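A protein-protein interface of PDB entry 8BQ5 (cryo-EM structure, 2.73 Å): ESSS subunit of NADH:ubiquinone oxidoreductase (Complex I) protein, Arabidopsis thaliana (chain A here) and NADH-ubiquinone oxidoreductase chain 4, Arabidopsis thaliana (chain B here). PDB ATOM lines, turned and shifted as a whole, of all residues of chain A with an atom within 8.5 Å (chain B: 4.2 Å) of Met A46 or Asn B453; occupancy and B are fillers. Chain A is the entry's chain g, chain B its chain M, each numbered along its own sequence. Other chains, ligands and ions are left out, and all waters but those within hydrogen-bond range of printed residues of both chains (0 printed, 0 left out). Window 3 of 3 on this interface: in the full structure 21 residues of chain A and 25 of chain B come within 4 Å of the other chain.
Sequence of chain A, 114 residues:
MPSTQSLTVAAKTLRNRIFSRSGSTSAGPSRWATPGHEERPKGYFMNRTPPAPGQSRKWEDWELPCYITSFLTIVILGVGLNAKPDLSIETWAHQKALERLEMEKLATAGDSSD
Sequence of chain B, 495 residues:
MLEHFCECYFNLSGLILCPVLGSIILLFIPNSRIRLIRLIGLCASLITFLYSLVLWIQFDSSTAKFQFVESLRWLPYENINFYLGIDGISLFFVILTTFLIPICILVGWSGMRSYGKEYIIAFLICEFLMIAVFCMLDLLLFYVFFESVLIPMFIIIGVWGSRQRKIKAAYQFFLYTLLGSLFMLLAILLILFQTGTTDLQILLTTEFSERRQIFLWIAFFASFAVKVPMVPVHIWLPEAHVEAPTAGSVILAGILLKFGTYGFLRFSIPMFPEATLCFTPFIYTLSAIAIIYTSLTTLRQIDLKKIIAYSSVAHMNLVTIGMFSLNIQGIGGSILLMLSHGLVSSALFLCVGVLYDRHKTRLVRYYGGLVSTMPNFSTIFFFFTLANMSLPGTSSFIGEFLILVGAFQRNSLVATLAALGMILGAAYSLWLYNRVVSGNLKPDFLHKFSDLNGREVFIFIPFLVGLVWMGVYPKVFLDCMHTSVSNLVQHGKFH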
ATOM      1  N   GLY A  43      18.933 -22.024 -16.979  1.00  0.00           N
ATOM      2  CA  GLY A  43      17.765 -21.739 -17.784  1.00  0.00           C
ATOM      3  C   GLY A  43      17.604 -20.253 -18.039  1.00  0.00           C
ATOM      4  O   GLY A  43      18.441 -19.425 -17.677  1.00  0.00           O
ATOM      5  N   TYR A  44      16.488 -19.912 -18.677  1.00  0.00           N
ATOM      6  CA  TYR A  44      16.147 -18.527 -18.967  1.00  0.00           C
ATOM      7  C   TYR A  44      14.736 -18.240 -18.487  1.00  0.00           C
ATOM      8  O   TYR A  44      13.855 -19.101 -18.571  1.00  0.00           O
ATOM      9  CB  TYR A  44      16.263 -18.222 -20.463  1.00  0.00           C
ATOM     10  CG  TYR A  44      17.662 -18.400 -21.003  1.00  0.00           C
ATOM     11  CD1 TYR A  44      18.676 -17.519 -20.656  1.00  0.00           C
ATOM     12  CD2 TYR A  44      17.969 -19.457 -21.847  1.00  0.00           C
ATOM     13  CE1 TYR A  44      19.956 -17.682 -21.140  1.00  0.00           C
ATOM     14  CE2 TYR A  44      19.245 -19.626 -22.337  1.00  0.00           C
ATOM     15  CZ  TYR A  44      20.234 -18.737 -21.981  1.00  0.00           C
ATOM     16  OH  TYR A  44      21.509 -18.904 -22.468  1.00  0.00           O
ATOM     17  N   PHE A  45      14.527 -17.026 -17.984  1.00  0.00           N
ATOM     18  CA  PHE A  45      13.209 -16.623 -17.515  1.00  0.00           C
ATOM     19  C   PHE A  45      12.210 -16.658 -18.663  1.00  0.00           C
ATOM     20  O   PHE A  45      12.389 -15.972 -19.674  1.00  0.00           O
ATOM     21  CB  PHE A  45      13.280 -15.224 -16.905  1.00  0.00           C
ATOM     22  CG  PHE A  45      11.973 -14.738 -16.354  1.00  0.00           C
ATOM     23  CD1 PHE A  45      11.254 -15.512 -15.462  1.00  0.00           C
ATOM     24  CD2 PHE A  45      11.469 -13.502 -16.716  1.00  0.00           C
ATOM     25  CE1 PHE A  45      10.052 -15.069 -14.946  1.00  0.00           C
ATOM     26  CE2 PHE A  45      10.270 -13.051 -16.204  1.00  0.00           C
ATOM     27  CZ  PHE A  45       9.559 -13.838 -15.318  1.00  0.00           C
ATOM     28  N   MET A  46      11.162 -17.468 -18.503  1.00  0.00           N
ATOM     29  CA  MET A  46      10.116 -17.635 -19.515  1.00  0.00           C
ATOM     30  C   MET A  46      10.670 -18.181 -20.828  1.00  0.00           C
ATOM     31  O   MET A  46      10.111 -17.937 -21.900  1.00  0.00           O
ATOM     32  CB  MET A  46       9.345 -16.330 -19.739  1.00  0.00           C
ATOM     33  CG  MET A  46       8.461 -15.946 -18.558  1.00  0.00           C
ATOM     34  SD  MET A  46       8.045 -14.195 -18.444  1.00  0.00           S
ATOM     35  CE  MET A  46       8.626 -13.599 -20.024  1.00  0.00           C
ATOM     36  N   ASN A  47      11.780 -18.918 -20.740  1.00  0.00           N
ATOM     37  CA  ASN A  47      12.297 -19.749 -21.830  1.00  0.00           C
ATOM     38  C   ASN A  47      12.473 -18.978 -23.135  1.00  0.00           C
ATOM     39  O   ASN A  47      12.174 -19.493 -24.214  1.00  0.00           O
ATOM     40  CB  ASN A  47      11.403 -20.970 -22.057  1.00  0.00           C
ATOM     41  CG  ASN A  47      11.641 -22.056 -21.034  1.00  0.00           C
ATOM     42  OD1 ASN A  47      11.023 -22.073 -19.971  1.00  0.00           O
ATOM     43  ND2 ASN A  47      12.529 -22.983 -21.359  1.00  0.00           N
ATOM     44  N   ARG A  48      12.961 -17.747 -23.056  1.00  0.00           N
ATOM     45  CA  ARG A  48      13.314 -16.969 -24.234  1.00  0.00           C
ATOM     46  C   ARG A  48      14.819 -16.744 -24.248  1.00  0.00           C
ATOM     47  O   ARG A  48      15.397 -16.313 -23.245  1.00  0.00           O
ATOM     48  CB  ARG A  48      12.568 -15.634 -24.260  1.00  0.00           C
ATOM     49  CG  ARG A  48      12.595 -14.883 -22.948  1.00  0.00           C
ATOM     50  CD  ARG A  48      12.211 -13.432 -23.144  1.00  0.00           C
ATOM     51  NE  ARG A  48      10.791 -13.272 -23.435  1.00  0.00           N
ATOM     52  CZ  ARG A  48      10.016 -12.352 -22.879  1.00  0.00           C
ATOM     53  NH1 ARG A  48      10.491 -11.496 -21.990  1.00  0.00           N
ATOM     54  NH2 ARG A  48       8.733 -12.292 -23.221  1.00  0.00           N
ATOM     55  N   THR A  49      15.452 -17.058 -25.374  1.00  0.00           N
ATOM     56  CA  THR A  49      16.878 -16.821 -25.510  1.00  0.00           C
ATOM     57  C   THR A  49      17.165 -15.320 -25.512  1.00  0.00           C
ATOM     58  O   THR A  49      16.447 -14.543 -26.147  1.00  0.00           O
ATOM     59  CB  THR A  49      17.410 -17.449 -26.795  1.00  0.00           C
ATOM     60  OG1 THR A  49      16.667 -16.949 -27.913  1.00  0.00           O
ATOM     61  CG2 THR A  49      17.286 -18.962 -26.739  1.00  0.00           C
ATOM     62  N   ARG A  57      15.563  -6.875 -26.471  1.00  0.00           N
ATOM     63  CA  ARG A  57      14.489  -7.757 -26.903  1.00  0.00           C
ATOM     64  C   ARG A  57      13.425  -6.968 -27.654  1.00  0.00           C
ATOM     65  O   ARG A  57      13.095  -5.835 -27.294  1.00  0.00           O
ATOM     66  CB  ARG A  57      13.871  -8.460 -25.696  1.00  0.00           C
ATOM     67  CG  ARG A  57      12.625  -9.276 -26.001  1.00  0.00           C
ATOM     68  CD  ARG A  57      12.049  -9.884 -24.736  1.00  0.00           C
ATOM     69  NE  ARG A  57      11.351  -8.899 -23.918  1.00  0.00           N
ATOM     70  CZ  ARG A  57      10.046  -8.675 -23.971  1.00  0.00           C
ATOM     71  NH1 ARG A  57       9.262  -9.352 -24.793  1.00  0.00           N
ATOM     72  NH2 ARG A  57       9.514  -7.751 -23.177  1.00  0.00           N
ATOM     73  N   GLU A  60       6.727  -8.176 -28.487  1.00  0.00           N
ATOM     74  CA  GLU A  60       5.662  -8.690 -29.331  1.00  0.00           C
ATOM     75  C   GLU A  60       4.491  -7.713 -29.357  1.00  0.00           C
ATOM     76  O   GLU A  60       4.342  -6.851 -28.487  1.00  0.00           O
ATOM     77  CB  GLU A  60       5.194 -10.063 -28.848  1.00  0.00           C
ATOM     78  CG  GLU A  60       6.311 -11.053 -28.609  1.00  0.00           C
ATOM     79  CD  GLU A  60       6.012 -12.418 -29.194  1.00  0.00           C
ATOM     80  OE1 GLU A  60       6.784 -12.873 -30.063  1.00  0.00           O
ATOM     81  OE2 GLU A  60       5.004 -13.034 -28.790  1.00  0.00           O
ATOM     82  N   TRP A  62       1.380  -7.822 -28.739  1.00  0.00           N
ATOM     83  CA  TRP A  62       0.394  -7.780 -27.668  1.00  0.00           C
ATOM     84  C   TRP A  62       0.899  -7.078 -26.413  1.00  0.00           C
ATOM     85  O   TRP A  62       0.081  -6.667 -25.585  1.00  0.00           O
ATOM     86  CB  TRP A  62      -0.048  -9.201 -27.315  1.00  0.00           C
ATOM     87  CG  TRP A  62       1.086 -10.063 -26.885  1.00  0.00           C
ATOM     88  CD1 TRP A  62       1.841 -10.876 -27.674  1.00  0.00           C
ATOM     89  CD2 TRP A  62       1.605 -10.197 -25.558  1.00  0.00           C
ATOM     90  NE1 TRP A  62       2.800 -11.506 -26.924  1.00  0.00           N
ATOM     91  CE2 TRP A  62       2.674 -11.108 -25.619  1.00  0.00           C
ATOM     92  CE3 TRP A  62       1.265  -9.637 -24.323  1.00  0.00           C
ATOM     93  CZ2 TRP A  62       3.413 -11.465 -24.499  1.00  0.00           C
ATOM     94  CZ3 TRP A  62       1.997  -9.995 -23.209  1.00  0.00           C
ATOM     95  CH2 TRP A  62       3.057 -10.904 -23.304  1.00  0.00           C
ATOM     96  N   GLU A  63       2.215  -6.927 -26.256  1.00  0.00           N
ATOM     97  CA  GLU A  63       2.771  -6.491 -24.977  1.00  0.00           C
ATOM     98  C   GLU A  63       2.357  -5.063 -24.640  1.00  0.00           C
ATOM     99  O   GLU A  63       1.873  -4.791 -23.536  1.00  0.00           O
ATOM    100  CB  GLU A  63       4.294  -6.622 -24.997  1.00  0.00           C
ATOM    101  CG  GLU A  63       4.776  -8.039 -25.225  1.00  0.00           C
ATOM    102  CD  GLU A  63       6.108  -8.318 -24.566  1.00  0.00           C
ATOM    103  OE1 GLU A  63       6.301  -7.900 -23.404  1.00  0.00           O
ATOM    104  OE2 GLU A  63       6.965  -8.952 -25.213  1.00  0.00           O
ATOM    105  N   TYR A  67       0.095  -4.050 -21.544  1.00  0.00           N
ATOM    106  CA  TYR A  67       0.746  -3.356 -20.437  1.00  0.00           C
ATOM    107  C   TYR A  67       0.081  -2.015 -20.161  1.00  0.00           C
ATOM    108  O   TYR A  67      -0.053  -1.609 -19.001  1.00  0.00           O
ATOM    109  CB  TYR A  67       2.232  -3.165 -20.735  1.00  0.00           C
ATOM    110  CG  TYR A  67       3.026  -4.450 -20.755  1.00  0.00           C
ATOM    111  CD1 TYR A  67       2.511  -5.614 -20.204  1.00  0.00           C
ATOM    112  CD2 TYR A  67       4.286  -4.499 -21.332  1.00  0.00           C
ATOM    113  CE1 TYR A  67       3.229  -6.790 -20.224  1.00  0.00           C
ATOM    114  CE2 TYR A  67       5.012  -5.670 -21.356  1.00  0.00           C
ATOM    115  CZ  TYR A  67       4.478  -6.813 -20.800  1.00  0.00           C
ATOM    116  OH  TYR A  67       5.195  -7.985 -20.818  1.00  0.00           O
ATOM    117  N   ASP B 451       8.462 -24.592 -20.597  1.00  0.00           N
ATOM    118  CA  ASP B 451       7.658 -23.895 -19.606  1.00  0.00           C
ATOM    119  C   ASP B 451       6.901 -22.740 -20.265  1.00  0.00           C
ATOM    120  O   ASP B 451       6.984 -22.510 -21.475  1.00  0.00           O
ATOM    121  CB  ASP B 451       8.539 -23.406 -18.460  1.00  0.00           C
ATOM    122  CG  ASP B 451       7.840 -23.462 -17.121  1.00  0.00           C
ATOM    123  OD1 ASP B 451       6.594 -23.491 -17.103  1.00  0.00           O
ATOM    124  OD2 ASP B 451       8.536 -23.482 -16.085  1.00  0.00           O
ATOM    125  N   LEU B 452       6.146 -22.003 -19.453  1.00  0.00           N
ATOM    126  CA  LEU B 452       5.300 -20.936 -19.971  1.00  0.00           C
ATOM    127  C   LEU B 452       6.133 -19.817 -20.582  1.00  0.00           C
ATOM    128  O   LEU B 452       7.169 -19.423 -20.041  1.00  0.00           O
ATOM    129  CB  LEU B 452       4.415 -20.366 -18.864  1.00  0.00           C
ATOM    130  CG  LEU B 452       3.742 -21.327 -17.886  1.00  0.00           C
ATOM    131  CD1 LEU B 452       3.361 -20.580 -16.624  1.00  0.00           C
ATOM    132  CD2 LEU B 452       2.518 -21.974 -18.510  1.00  0.00           C
ATOM    133  N   ASN B 453       5.668 -19.300 -21.716  1.00  0.00           N
ATOM    134  CA  ASN B 453       6.323 -18.168 -22.350  1.00  0.00           C
ATOM    135  C   ASN B 453       5.809 -16.864 -21.744  1.00  0.00           C
ATOM    136  O   ASN B 453       5.020 -16.853 -20.796  1.00  0.00           O
ATOM    137  CB  ASN B 453       6.120 -18.206 -23.867  1.00  0.00           C
ATOM    138  CG  ASN B 453       4.657 -18.197 -24.277  1.00  0.00           C
ATOM    139  OD1 ASN B 453       3.770 -17.874 -23.489  1.00  0.00           O
ATOM    140  ND2 ASN B 453       4.401 -18.542 -25.531  1.00  0.00           N
ATOM    141  N   GLY B 454       6.258 -15.745 -22.313  1.00  0.00           N
ATOM    142  CA  GLY B 454       5.874 -14.449 -21.780  1.00  0.00           C
ATOM    143  C   GLY B 454       4.392 -14.164 -21.907  1.00  0.00           C
ATOM    144  O   GLY B 454       3.798 -13.524 -21.037  1.00  0.00           O
ATOM    145  N   ARG B 455       3.778 -14.615 -23.001  1.00  0.00           N
ATOM    146  CA  ARG B 455       2.349 -14.387 -23.185  1.00  0.00           C
ATOM    147  C   ARG B 455       1.531 -15.222 -22.215  1.00  0.00           C
ATOM    148  O   ARG B 455       0.539 -14.743 -21.652  1.00  0.00           O
ATOM    149  CB  ARG B 455       1.948 -14.696 -24.625  1.00  0.00           C
ATOM    150  CG  ARG B 455       0.550 -14.235 -24.983  1.00  0.00           C
ATOM    151  CD  ARG B 455       0.240 -14.501 -26.446  1.00  0.00           C
ATOM    152  NE  ARG B 455       0.976 -15.651 -26.959  1.00  0.00           N
ATOM    153  CZ  ARG B 455       0.519 -16.896 -26.946  1.00  0.00           C
ATOM    154  NH1 ARG B 455      -0.683 -17.186 -26.478  1.00  0.00           N
ATOM    155  NH2 ARG B 455       1.290 -17.873 -27.415  1.00  0.00           N
ATOM    156  N   GLU B 456       1.928 -16.476 -22.010  1.00  0.00           N
ATOM    157  CA  GLU B 456       1.199 -17.346 -21.097  1.00  0.00           C
ATOM    158  C   GLU B 456       1.320 -16.861 -19.659  1.00  0.00           C
ATOM    159  O   GLU B 456       0.370 -16.980 -18.879  1.00  0.00           O
ATOM    160  CB  GLU B 456       1.701 -18.782 -21.237  1.00  0.00           C
ATOM    161  CG  GLU B 456       1.144 -19.495 -22.458  1.00  0.00           C
ATOM    162  CD  GLU B 456       2.060 -20.582 -22.982  1.00  0.00           C
ATOM    163  OE1 GLU B 456       3.232 -20.636 -22.556  1.00  0.00           O
ATOM    164  OE2 GLU B 456       1.606 -21.385 -23.822  1.00  0.00           O
ATOM    165  N   VAL B 457       2.480 -16.315 -19.290  1.00  0.00           N
ATOM    166  CA  VAL B 457       2.653 -15.791 -17.938  1.00  0.00           C
ATOM    167  C   VAL B 457       1.742 -14.588 -17.717  1.00  0.00           C
ATOM    168  O   VAL B 457       1.081 -14.472 -16.678  1.00  0.00           O
ATOM    169  CB  VAL B 457       4.130 -15.442 -17.679  1.00  0.00           C
ATOM    170  CG1 VAL B 457       4.265 -14.604 -16.417  1.00  0.00           C
ATOM    171  CG2 VAL B 457       4.956 -16.707 -17.568  1.00  0.00           C
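OD1 of Asn B453 lies close to N of Arg B455 (3.3 Å).
The side-chain amide oxygen of Asn B453 is in hydrogen-bond range of the backbone NH of Glu B456.
OE2 of Glu A60 lies within hydrogen-bond range of NE1 of Trp A62 (3.3 Å).
Of chain B, only Leu B452, Asn B453, Gly B454 and Val B457 come within 4 Å of Met A46.
Printed residues of chain B within 4 Å of Asn A47: Asp B451 (3.2 Å).
Printed residues of chain B within 4 Å of Arg A48: Gly B454.
Of the printed residues of chain A, Asp B451 touches Asn A47 (3.2 Å).
Asn B453 touches just one residue of chain A: Met A46.
Printed residues of chain A within 4 Å of Arg B455: Trp A62 (3.4 Å).
Printed residues of chain A within 4 Å of Val B457: Met A46.
The nearest printed residue of chain B that does not touch Met A46 is Asp B451 (5.6 Å).
Printed residues of chain B that touch a printed residue of chain A: Asp B451, Leu B452, Asn B453, Gly B454, Arg B455 and Val B457.
Of the 12 printed residues of chain A, 4 touch a printed residue of chain B.
Among the printed residues, 8 pairs touch across the chains.
Among the printed residues, no Asp or Glu carboxylate lies within 4 Å of a Lys or Arg side-chain nitrogen of the other chain.
Among the printed residues, pairs that only touch across the chains: Asn A47 with Asp B451 (3.2 Å), Met A46 with Gly B454 (3.4 Å), Trp A62 with Arg B455 (3.4 Å), Met A46 with Leu B452 (3.5 Å), Trp A62 with Gly B454 (3.5 Å), Met A46 with Val B457 (3.7 Å), Met A46 with Asn B453 (3.8 Å) and Arg A48 with Gly B454 (3.9 Å).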
